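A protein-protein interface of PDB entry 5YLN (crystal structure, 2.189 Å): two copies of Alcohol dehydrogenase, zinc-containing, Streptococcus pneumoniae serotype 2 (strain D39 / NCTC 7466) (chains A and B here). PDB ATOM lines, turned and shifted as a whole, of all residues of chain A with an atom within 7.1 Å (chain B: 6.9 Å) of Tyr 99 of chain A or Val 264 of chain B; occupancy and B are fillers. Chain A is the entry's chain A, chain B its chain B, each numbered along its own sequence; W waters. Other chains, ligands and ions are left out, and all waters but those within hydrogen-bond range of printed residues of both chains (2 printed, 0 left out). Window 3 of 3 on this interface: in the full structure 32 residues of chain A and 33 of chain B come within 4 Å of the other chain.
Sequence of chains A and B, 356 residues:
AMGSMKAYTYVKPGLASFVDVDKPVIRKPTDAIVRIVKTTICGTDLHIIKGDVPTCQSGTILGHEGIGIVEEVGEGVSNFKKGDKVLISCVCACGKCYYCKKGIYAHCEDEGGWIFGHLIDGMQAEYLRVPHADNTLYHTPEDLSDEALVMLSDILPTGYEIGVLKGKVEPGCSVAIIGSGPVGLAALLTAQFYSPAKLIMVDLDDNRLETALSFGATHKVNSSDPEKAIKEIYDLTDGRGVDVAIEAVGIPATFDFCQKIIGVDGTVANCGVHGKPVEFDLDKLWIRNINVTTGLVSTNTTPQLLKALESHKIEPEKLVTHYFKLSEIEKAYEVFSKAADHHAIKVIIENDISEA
A ring nitrogen (NE2) of His 107 of chain A sits at hydrogen-bond distance from the side-chain amide oxygen of Asn 289 of chain B, 3.1 Å away.
The side-chain carboxylate (OE1) of Glu 109 of chain A lies within salt-bridge range of the guanidinium group (NE) of Arg 240 of chain B, 2.9 Å away.
A ring nitrogen (NE2) of His 107 of chain A lies within hydrogen-bond range of the backbone carbonyl oxygen (O) of Ile 287 of chain B.
The backbone carbonyl oxygen (O) of Arg 240 of chain B sits at hydrogen-bond distance from the guanidinium group (NH2) of Arg 288 of chain B, at 3.4 Å.
SG of Cys 97 of chain A sits close to N of Glu 109 of chain A.
The backbone NH of Asp 265 of chain B sits at hydrogen-bond distance from the backbone carbonyl oxygen of Arg 288 of chain B (3.5 Å).
The backbone carbonyl oxygen (O) of Tyr 99 of chain A lies within hydrogen-bond range of the backbone NH (N) of Ile 104 of chain A (3.0 Å).
NE of Arg 288 of chain B sits at hydrogen-bond distance from O of Ile 262 of chain B.
The backbone carbonyl oxygen of Asn 289 of chain B lies within hydrogen-bond range of the backbone NH of Asp 265 of chain B, at 2.9 Å.
Among the printed residues, pairs that only touch across the chains: Tyr 98 of chain A with Arg 240 of chain B (3.7 Å), Tyr 99 of chain A with Arg 240 of chain B (3.3 Å), Tyr 99 of chain A with Val 264 of chain B (3.7 Å), Ile 104 of chain A with Asp 265 of chain B (3.7 Å), His 107 of chain A with Val 264 of chain B (3.5 Å) and His 107 of chain A with Arg 288 of chain B (3.9 Å).
Printed residues of chain B within 4 Å of Tyr 98 of chain A: Arg 240 (3.7 Å).
Of chain B, only Arg 240 and Val 264 come within 4 Å of Tyr 99 of chain A.
Of the printed residues of chain B, Ile 104 of chain A touches Asp 265 (3.7 Å).
Of the printed residues of chain B, Glu 109 of chain A touches Arg 240 (2.9 Å).
Val 264 of chain B touches just these residues of chain A: Tyr 99 (3.7 Å) and His 107 (3.5 Å).
Of the printed residues of chain A, Arg 288 of chain B touches His 107 (3.9 Å).
Of the printed residues of chain A, Asn 289 of chain B touches His 107 (3.1 Å).
The nearest residue of chain B that does not touch Tyr 99 of chain A is Gly 263 of chain B (5.3 Å).
Hydrophobic or aromatic side chains of chain B within 4 Å of the printed part of chain A: Val 264.
Of the 15 printed residues of chain A, 5 touch a printed residue of chain B.
Among the printed residues, Asp or Glu carboxylates within 4 Å of a Lys or Arg side-chain nitrogen of the other chain: Glu 109 of chain A with Arg 240 of chain B (2.9 Å).
No position is printed for both chains.
Of the 9 pairs that touch across the chains among the printed residues, none has its exchanged pair printed and touching as well.
Water W1 lies within hydrogen-bond range of the side-chain hydroxyl (OG) of Ser 298 of chain A and the side-chain amide nitrogen (ND2) of Asn 289 of chain B.
Water W2 lies within hydrogen-bond range of OH of Tyr 99 of chain A (2.7 Å), O of Arg 240 of chain B (2.9 Å) and N of Val 264 of chain B (2.9 Å).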
ATOM      1  N   LYS A  96      -5.930  12.806  -1.704  1.00  0.00           N
ATOM      2  CA  LYS A  96      -4.637  12.142  -1.753  1.00  0.00           C
ATOM      3  C   LYS A  96      -4.697  10.624  -1.858  1.00  0.00           C
ATOM      4  O   LYS A  96      -3.670  10.012  -2.163  1.00  0.00           O
ATOM      5  CB  LYS A  96      -3.805  12.481  -0.504  1.00  0.00           C
ATOM      6  CG  LYS A  96      -3.297  13.902  -0.394  1.00  0.00           C
ATOM      7  CD  LYS A  96      -2.761  14.121   1.023  1.00  0.00           C
ATOM      8  CE  LYS A  96      -1.866  15.343   1.129  1.00  0.00           C
ATOM      9  NZ  LYS A  96      -1.448  15.517   2.548  1.00  0.00           N
ATOM     10  N   CYS A  97      -5.832   9.991  -1.584  1.00  0.00           N
ATOM     11  CA  CYS A  97      -5.846   8.538  -1.481  1.00  0.00           C
ATOM     12  C   CYS A  97      -6.054   7.899  -2.857  1.00  0.00           C
ATOM     13  O   CYS A  97      -6.208   8.576  -3.873  1.00  0.00           O
ATOM     14  CB  CYS A  97      -6.935   8.085  -0.519  1.00  0.00           C
ATOM     15  SG  CYS A  97      -8.574   8.344  -1.233  1.00  0.00           S
ATOM     16  N   TYR A  98      -6.111   6.566  -2.867  1.00  0.00           N
ATOM     17  CA  TYR A  98      -6.250   5.809  -4.106  1.00  0.00           C
ATOM     18  C   TYR A  98      -7.451   6.289  -4.925  1.00  0.00           C
ATOM     19  O   TYR A  98      -7.352   6.479  -6.143  1.00  0.00           O
ATOM     20  CB  TYR A  98      -6.347   4.313  -3.773  1.00  0.00           C
ATOM     21  CG  TYR A  98      -6.542   3.401  -4.959  1.00  0.00           C
ATOM     22  CD1 TYR A  98      -7.810   3.156  -5.465  1.00  0.00           C
ATOM     23  CD2 TYR A  98      -5.459   2.779  -5.570  1.00  0.00           C
ATOM     24  CE1 TYR A  98      -8.001   2.332  -6.548  1.00  0.00           C
ATOM     25  CE2 TYR A  98      -5.640   1.940  -6.663  1.00  0.00           C
ATOM     26  CZ  TYR A  98      -6.918   1.722  -7.143  1.00  0.00           C
ATOM     27  OH  TYR A  98      -7.123   0.904  -8.224  1.00  0.00           O
ATOM     28  N   TYR A  99      -8.593   6.528  -4.262  1.00  0.00           N
ATOM     29  CA  TYR A  99      -9.799   6.873  -5.010  1.00  0.00           C
ATOM     30  C   TYR A  99      -9.901   8.361  -5.289  1.00  0.00           C
ATOM     31  O   TYR A  99     -10.427   8.745  -6.337  1.00  0.00           O
ATOM     32  CB  TYR A  99     -11.049   6.353  -4.286  1.00  0.00           C
ATOM     33  CG  TYR A  99     -11.142   4.859  -4.434  1.00  0.00           C
ATOM     34  CD1 TYR A  99     -11.190   4.288  -5.708  1.00  0.00           C
ATOM     35  CD2 TYR A  99     -11.126   4.012  -3.321  1.00  0.00           C
ATOM     36  CE1 TYR A  99     -11.250   2.915  -5.871  1.00  0.00           C
ATOM     37  CE2 TYR A  99     -11.181   2.643  -3.472  1.00  0.00           C
ATOM     38  CZ  TYR A  99     -11.232   2.100  -4.758  1.00  0.00           C
ATOM     39  OH  TYR A  99     -11.287   0.751  -4.936  1.00  0.00           O
ATOM     40  N   CYS A 100      -9.417   9.209  -4.377  1.00  0.00           N
ATOM     41  CA  CYS A 100      -9.389  10.647  -4.647  1.00  0.00           C
ATOM     42  C   CYS A 100      -8.501  10.968  -5.847  1.00  0.00           C
ATOM     43  O   CYS A 100      -8.790  11.892  -6.619  1.00  0.00           O
ATOM     44  CB  CYS A 100      -8.906  11.411  -3.415  1.00  0.00           C
ATOM     45  SG  CYS A 100     -10.166  11.623  -2.120  1.00  0.00           S
ATOM     46  N   LYS A 101      -7.403  10.235  -6.004  1.00  0.00           N
ATOM     47  CA  LYS A 101      -6.560  10.447  -7.176  1.00  0.00           C
ATOM     48  C   LYS A 101      -7.299  10.137  -8.475  1.00  0.00           C
ATOM     49  O   LYS A 101      -6.947  10.687  -9.519  1.00  0.00           O
ATOM     50  CB  LYS A 101      -5.280   9.615  -7.050  1.00  0.00           C
ATOM     51  CG  LYS A 101      -4.262  10.245  -6.098  1.00  0.00           C
ATOM     52  CD  LYS A 101      -3.858  11.639  -6.593  1.00  0.00           C
ATOM     53  CE  LYS A 101      -2.728  12.227  -5.781  1.00  0.00           C
ATOM     54  NZ  LYS A 101      -1.623  11.250  -5.607  1.00  0.00           N
ATOM     55  N   LYS A 102      -8.336   9.304  -8.426  1.00  0.00           N
ATOM     56  CA  LYS A 102      -9.164   9.019  -9.587  1.00  0.00           C
ATOM     57  C   LYS A 102     -10.339   9.980  -9.733  1.00  0.00           C
ATOM     58  O   LYS A 102     -11.077   9.877 -10.716  1.00  0.00           O
ATOM     59  CB  LYS A 102      -9.693   7.582  -9.522  1.00  0.00           C
ATOM     60  CG  LYS A 102      -8.614   6.500  -9.590  1.00  0.00           C
ATOM     61  CD  LYS A 102      -9.221   5.107  -9.418  1.00  0.00           C
ATOM     62  CE  LYS A 102      -8.175   4.012  -9.594  1.00  0.00           C
ATOM     63  NZ  LYS A 102      -7.706   3.894 -11.007  1.00  0.00           N
ATOM     64  N   GLY A 103     -10.528  10.919  -8.806  1.00  0.00           N
ATOM     65  CA  GLY A 103     -11.730  11.736  -8.825  1.00  0.00           C
ATOM     66  C   GLY A 103     -12.981  11.054  -8.290  1.00  0.00           C
ATOM     67  O   GLY A 103     -14.079  11.625  -8.383  1.00  0.00           O
ATOM     68  N   ILE A 104     -12.845   9.868  -7.701  1.00  0.00           N
ATOM     69  CA  ILE A 104     -13.974   9.117  -7.163  1.00  0.00           C
ATOM     70  C   ILE A 104     -14.117   9.463  -5.684  1.00  0.00           C
ATOM     71  O   ILE A 104     -13.877   8.628  -4.808  1.00  0.00           O
ATOM     72  CB  ILE A 104     -13.780   7.606  -7.399  1.00  0.00           C
ATOM     73  CG1 ILE A 104     -13.447   7.352  -8.880  1.00  0.00           C
ATOM     74  CG2 ILE A 104     -15.014   6.810  -6.997  1.00  0.00           C
ATOM     75  CD1 ILE A 104     -13.100   5.919  -9.154  1.00  0.00           C
ATOM     76  N   TYR A 105     -14.503  10.709  -5.396  1.00  0.00           N
ATOM     77  CA  TYR A 105     -14.528  11.165  -4.011  1.00  0.00           C
ATOM     78  C   TYR A 105     -15.547  10.397  -3.181  1.00  0.00           C
ATOM     79  O   TYR A 105     -15.415  10.343  -1.955  1.00  0.00           O
ATOM     80  CB  TYR A 105     -14.808  12.671  -3.940  1.00  0.00           C
ATOM     81  CG  TYR A 105     -13.827  13.511  -4.753  1.00  0.00           C
ATOM     82  CD1 TYR A 105     -12.478  13.164  -4.834  1.00  0.00           C
ATOM     83  CD2 TYR A 105     -14.257  14.630  -5.460  1.00  0.00           C
ATOM     84  CE1 TYR A 105     -11.580  13.911  -5.579  1.00  0.00           C
ATOM     85  CE2 TYR A 105     -13.363  15.384  -6.220  1.00  0.00           C
ATOM     86  CZ  TYR A 105     -12.025  15.024  -6.276  1.00  0.00           C
ATOM     87  OH  TYR A 105     -11.118  15.767  -7.025  1.00  0.00           O
ATOM     88  N   ALA A 106     -16.547   9.799  -3.837  1.00  0.00           N
ATOM     89  CA  ALA A 106     -17.514   8.934  -3.181  1.00  0.00           C
ATOM     90  C   ALA A 106     -16.853   7.791  -2.415  1.00  0.00           C
ATOM     91  O   ALA A 106     -17.474   7.230  -1.498  1.00  0.00           O
ATOM     92  CB  ALA A 106     -18.490   8.383  -4.232  1.00  0.00           C
ATOM     93  N   HIS A 107     -15.610   7.429  -2.758  1.00  0.00           N
ATOM     94  CA  HIS A 107     -14.980   6.302  -2.084  1.00  0.00           C
ATOM     95  C   HIS A 107     -13.624   6.667  -1.506  1.00  0.00           C
ATOM     96  O   HIS A 107     -12.754   5.809  -1.372  1.00  0.00           O
ATOM     97  CB  HIS A 107     -14.901   5.107  -3.025  1.00  0.00           C
ATOM     98  CG  HIS A 107     -16.258   4.580  -3.362  1.00  0.00           C
ATOM     99  ND1 HIS A 107     -16.960   3.758  -2.507  1.00  0.00           N
ATOM    100  CD2 HIS A 107     -17.085   4.833  -4.404  1.00  0.00           C
ATOM    101  CE1 HIS A 107     -18.145   3.492  -3.026  1.00  0.00           C
ATOM    102  NE2 HIS A 107     -18.242   4.125  -4.183  1.00  0.00           N
ATOM    103  N   CYS A 108     -13.455   7.932  -1.108  1.00  0.00           N
ATOM    104  CA  CYS A 108     -12.246   8.352  -0.407  1.00  0.00           C
ATOM    105  C   CYS A 108     -12.012   7.481   0.831  1.00  0.00           C
ATOM    106  O   CYS A 108     -12.939   7.204   1.597  1.00  0.00           O
ATOM    107  CB  CYS A 108     -12.362   9.834  -0.026  1.00  0.00           C
ATOM    108  SG  CYS A 108     -11.108  10.379   1.158  1.00  0.00           S
ATOM    109  N   GLU A 109     -10.763   7.050   1.028  1.00  0.00           N
ATOM    110  CA  GLU A 109     -10.414   6.083   2.072  1.00  0.00           C
ATOM    111  C   GLU A 109      -9.917   6.720   3.369  1.00  0.00           C
ATOM    112  O   GLU A 109      -9.500   5.999   4.275  1.00  0.00           O
ATOM    113  CB  GLU A 109      -9.349   5.102   1.562  1.00  0.00           C
ATOM    114  CG  GLU A 109      -9.747   4.340   0.300  1.00  0.00           C
ATOM    115  CD  GLU A 109      -8.690   3.325  -0.179  1.00  0.00           C
ATOM    116  OE1 GLU A 109      -9.075   2.186  -0.530  1.00  0.00           O
ATOM    117  OE2 GLU A 109      -7.488   3.665  -0.219  1.00  0.00           O
ATOM    118  N   SER A 298     -20.006  11.697  -6.540  1.00  0.00           N
ATOM    119  CA  SER A 298     -18.699  12.131  -6.052  1.00  0.00           C
ATOM    120  C   SER A 298     -18.605  13.636  -5.832  1.00  0.00           C
ATOM    121  O   SER A 298     -17.909  14.075  -4.907  1.00  0.00           O
ATOM    122  CB  SER A 298     -17.594  11.707  -7.028  1.00  0.00           C
ATOM    123  OG  SER A 298     -17.106  10.433  -6.666  1.00  0.00           O
ATOM    124  N   GLY B 239      -7.564  -5.838  -0.973  1.00  0.00           N
ATOM    125  CA  GLY B 239      -8.884  -5.683  -0.389  1.00  0.00           C
ATOM    126  C   GLY B 239      -9.824  -4.815  -1.193  1.00  0.00           C
ATOM    127  O   GLY B 239     -10.871  -4.412  -0.678  1.00  0.00           O
ATOM    128  N   ARG B 240      -9.492  -4.513  -2.450  1.00  0.00           N
ATOM    129  CA  ARG B 240     -10.330  -3.617  -3.233  1.00  0.00           C
ATOM    130  C   ARG B 240     -11.165  -4.331  -4.287  1.00  0.00           C
ATOM    131  O   ARG B 240     -12.141  -3.747  -4.770  1.00  0.00           O
ATOM    132  CB  ARG B 240      -9.475  -2.524  -3.903  1.00  0.00           C
ATOM    133  CG  ARG B 240      -8.755  -1.606  -2.900  1.00  0.00           C
ATOM    134  CD  ARG B 240      -8.503  -0.218  -3.483  1.00  0.00           C
ATOM    135  NE  ARG B 240      -7.744   0.630  -2.568  1.00  0.00           N
ATOM    136  CZ  ARG B 240      -6.418   0.576  -2.432  1.00  0.00           C
ATOM    137  NH1 ARG B 240      -5.700  -0.288  -3.150  1.00  0.00           N
ATOM    138  NH2 ARG B 240      -5.808   1.382  -1.570  1.00  0.00           N
ATOM    139  N   GLY B 241     -10.835  -5.567  -4.644  1.00  0.00           N
ATOM    140  CA  GLY B 241     -11.557  -6.247  -5.701  1.00  0.00           C
ATOM    141  C   GLY B 241     -11.022  -5.856  -7.064  1.00  0.00           C
ATOM    142  O   GLY B 241     -10.123  -5.031  -7.193  1.00  0.00           O
ATOM    143  N   VAL B 242     -11.594  -6.456  -8.100  1.00  0.00           N
ATOM    144  CA  VAL B 242     -11.032  -6.339  -9.433  1.00  0.00           C
ATOM    145  C   VAL B 242     -11.680  -5.190 -10.184  1.00  0.00           C
ATOM    146  O   VAL B 242     -12.849  -4.846  -9.977  1.00  0.00           O
ATOM    147  CB  VAL B 242     -11.168  -7.660 -10.213  1.00  0.00           C
ATOM    148  CG1 VAL B 242     -10.406  -8.737  -9.505  1.00  0.00           C
ATOM    149  CG2 VAL B 242     -12.645  -8.030 -10.387  1.00  0.00           C
ATOM    150  N   ASP B 243     -10.891  -4.589 -11.079  1.00  0.00           N
ATOM    151  CA  ASP B 243     -11.417  -3.554 -11.957  1.00  0.00           C
ATOM    152  C   ASP B 243     -12.340  -4.120 -13.030  1.00  0.00           C
ATOM    153  O   ASP B 243     -13.260  -3.428 -13.473  1.00  0.00           O
ATOM    154  CB  ASP B 243     -10.256  -2.802 -12.597  1.00  0.00           C
ATOM    155  CG  ASP B 243      -9.349  -2.165 -11.569  1.00  0.00           C
ATOM    156  OD1 ASP B 243      -9.876  -1.410 -10.719  1.00  0.00           O
ATOM    157  OD2 ASP B 243      -8.122  -2.432 -11.592  1.00  0.00           O
ATOM    158  N   ILE B 261     -16.950  -9.983  -6.439  1.00  0.00           N
ATOM    159  CA  ILE B 261     -15.532  -9.640  -6.452  1.00  0.00           C
ATOM    160  C   ILE B 261     -15.267  -8.291  -7.079  1.00  0.00           C
ATOM    161  O   ILE B 261     -14.130  -7.799  -7.000  1.00  0.00           O
ATOM    162  CB  ILE B 261     -14.699 -10.729  -7.159  1.00  0.00           C
ATOM    163  CG1 ILE B 261     -15.157 -10.908  -8.612  1.00  0.00           C
ATOM    164  CG2 ILE B 261     -14.806 -12.021  -6.398  1.00  0.00           C
ATOM    165  CD1 ILE B 261     -14.178 -11.702  -9.480  1.00  0.00           C
ATOM    166  N   ILE B 262     -16.259  -7.675  -7.706  1.00  0.00           N
ATOM    167  CA  ILE B 262     -16.001  -6.462  -8.474  1.00  0.00           C
ATOM    168  C   ILE B 262     -15.731  -5.304  -7.523  1.00  0.00           C
ATOM    169  O   ILE B 262     -16.394  -5.152  -6.492  1.00  0.00           O
ATOM    170  CB  ILE B 262     -17.168  -6.156  -9.437  1.00  0.00           C
ATOM    171  CG1 ILE B 262     -16.774  -5.037 -10.425  1.00  0.00           C
ATOM    172  CG2 ILE B 262     -18.435  -5.751  -8.700  1.00  0.00           C
ATOM    173  CD1 ILE B 262     -15.706  -5.449 -11.391  1.00  0.00           C
ATOM    174  N   GLY B 263     -14.737  -4.480  -7.870  1.00  0.00           N
ATOM    175  CA  GLY B 263     -14.354  -3.358  -7.046  1.00  0.00           C
ATOM    176  C   GLY B 263     -15.032  -2.051  -7.441  1.00  0.00           C
ATOM    177  O   GLY B 263     -15.738  -1.965  -8.436  1.00  0.00           O
ATOM    178  N   VAL B 264     -14.786  -1.023  -6.615  1.00  0.00           N
ATOM    179  CA  VAL B 264     -15.265   0.326  -6.909  1.00  0.00           C
ATOM    180  C   VAL B 264     -14.795   0.751  -8.296  1.00  0.00           C
ATOM    181  O   VAL B 264     -13.607   0.678  -8.611  1.00  0.00           O
ATOM    182  CB  VAL B 264     -14.783   1.312  -5.828  1.00  0.00           C
ATOM    183  CG1 VAL B 264     -15.033   2.762  -6.266  1.00  0.00           C
ATOM    184  CG2 VAL B 264     -15.467   1.053  -4.489  1.00  0.00           C
ATOM    185  N   ASP B 265     -15.734   1.220  -9.120  1.00  0.00           N
ATOM    186  CA  ASP B 265     -15.534   1.742 -10.478  1.00  0.00           C
ATOM    187  C   ASP B 265     -15.360   0.635 -11.512  1.00  0.00           C
ATOM    188  O   ASP B 265     -15.143   0.941 -12.687  1.00  0.00           O
ATOM    189  CB  ASP B 265     -14.349   2.712 -10.593  1.00  0.00           C
ATOM    190  CG  ASP B 265     -14.502   3.682 -11.761  1.00  0.00           C
ATOM    191  OD1 ASP B 265     -15.613   4.249 -11.906  1.00  0.00           O
ATOM    192  OD2 ASP B 265     -13.519   3.884 -12.522  1.00  0.00           O
ATOM    193  N   GLY B 266     -15.464  -0.622 -11.124  1.00  0.00           N
ATOM    194  CA  GLY B 266     -15.192  -1.705 -12.036  1.00  0.00           C
ATOM    195  C   GLY B 266     -16.398  -2.112 -12.866  1.00  0.00           C
ATOM    196  O   GLY B 266     -17.541  -1.706 -12.639  1.00  0.00           O
ATOM    197  N   THR B 267     -16.128  -2.960 -13.849  1.00  0.00           N
ATOM    198  CA  THR B 267     -17.152  -3.411 -14.778  1.00  0.00           C
ATOM    199  C   THR B 267     -17.242  -4.925 -14.722  1.00  0.00           C
ATOM    200  O   THR B 267     -16.218  -5.616 -14.782  1.00  0.00           O
ATOM    201  CB  THR B 267     -16.848  -2.916 -16.203  1.00  0.00           C
ATOM    202  OG1 THR B 267     -16.871  -1.477 -16.212  1.00  0.00           O
ATOM    203  CG2 THR B 267     -17.871  -3.450 -17.202  1.00  0.00           C
ATOM    204  N   ILE B 287     -24.105   1.713  -4.314  1.00  0.00           N
ATOM    205  CA  ILE B 287     -23.138   2.647  -3.759  1.00  0.00           C
ATOM    206  C   ILE B 287     -21.719   2.402  -4.257  1.00  0.00           C
ATOM    207  O   ILE B 287     -20.854   3.272  -4.083  1.00  0.00           O
ATOM    208  CB  ILE B 287     -23.222   2.567  -2.220  1.00  0.00           C
ATOM    209  CG1 ILE B 287     -22.769   3.887  -1.586  1.00  0.00           C
ATOM    210  CG2 ILE B 287     -22.429   1.357  -1.704  1.00  0.00           C
ATOM    211  CD1 ILE B 287     -22.902   3.918  -0.095  1.00  0.00           C
ATOM    212  N   ARG B 288     -21.457   1.275  -4.917  1.00  0.00           N
ATOM    213  CA  ARG B 288     -20.094   0.876  -5.263  1.00  0.00           C
ATOM    214  C   ARG B 288     -19.625   1.399  -6.616  1.00  0.00           C
ATOM    215  O   ARG B 288     -18.477   1.147  -6.997  1.00  0.00           O
ATOM    216  CB  ARG B 288     -19.981  -0.645  -5.228  1.00  0.00           C
ATOM    217  CG  ARG B 288     -18.559  -1.184  -5.132  1.00  0.00           C
ATOM    218  CD  ARG B 288     -18.645  -2.618  -4.671  1.00  0.00           C
ATOM    219  NE  ARG B 288     -17.367  -3.325  -4.652  1.00  0.00           N
ATOM    220  CZ  ARG B 288     -16.503  -3.267  -3.641  1.00  0.00           C
ATOM    221  NH1 ARG B 288     -16.760  -2.485  -2.588  1.00  0.00           N
ATOM    222  NH2 ARG B 288     -15.374  -3.970  -3.684  1.00  0.00           N
ATOM    223  N   ASN B 289     -20.470   2.127  -7.348  1.00  0.00           N
ATOM    224  CA  ASN B 289     -20.079   2.713  -8.631  1.00  0.00           C
ATOM    225  C   ASN B 289     -19.608   1.629  -9.603  1.00  0.00           C
ATOM    226  O   ASN B 289     -18.482   1.643 -10.095  1.00  0.00           O
ATOM    227  CB  ASN B 289     -18.986   3.786  -8.445  1.00  0.00           C
ATOM    228  CG  ASN B 289     -19.464   5.026  -7.694  1.00  0.00           C
ATOM    229  OD1 ASN B 289     -19.960   4.940  -6.572  1.00  0.00           O
ATOM    230  ND2 ASN B 289     -19.279   6.184  -8.300  1.00  0.00           N
ATOM    231  N   ILE B 290     -20.475   0.662  -9.870  1.00  0.00           N
ATOM    232  CA  ILE B 290     -20.107  -0.416 -10.775  1.00  0.00           C
ATOM    233  C   ILE B 290     -20.964  -0.352 -12.030  1.00  0.00           C
ATOM    234  O   ILE B 290     -21.946   0.388 -12.110  1.00  0.00           O
ATOM    235  CB  ILE B 290     -20.167  -1.805 -10.092  1.00  0.00           C
ATOM    236  CG1 ILE B 290     -21.559  -2.115  -9.519  1.00  0.00           C
ATOM    237  CG2 ILE B 290     -19.080  -1.879  -9.013  1.00  0.00           C
ATOM    238  CD1 ILE B 290     -22.486  -2.824 -10.486  1.00  0.00           C
HETATM  239  O   HOH W   1     -18.789   9.036  -7.996  1.00  0.00           O
HETATM  240  O   HOH W   2     -13.137  -1.098  -4.221  1.00  0.00           O
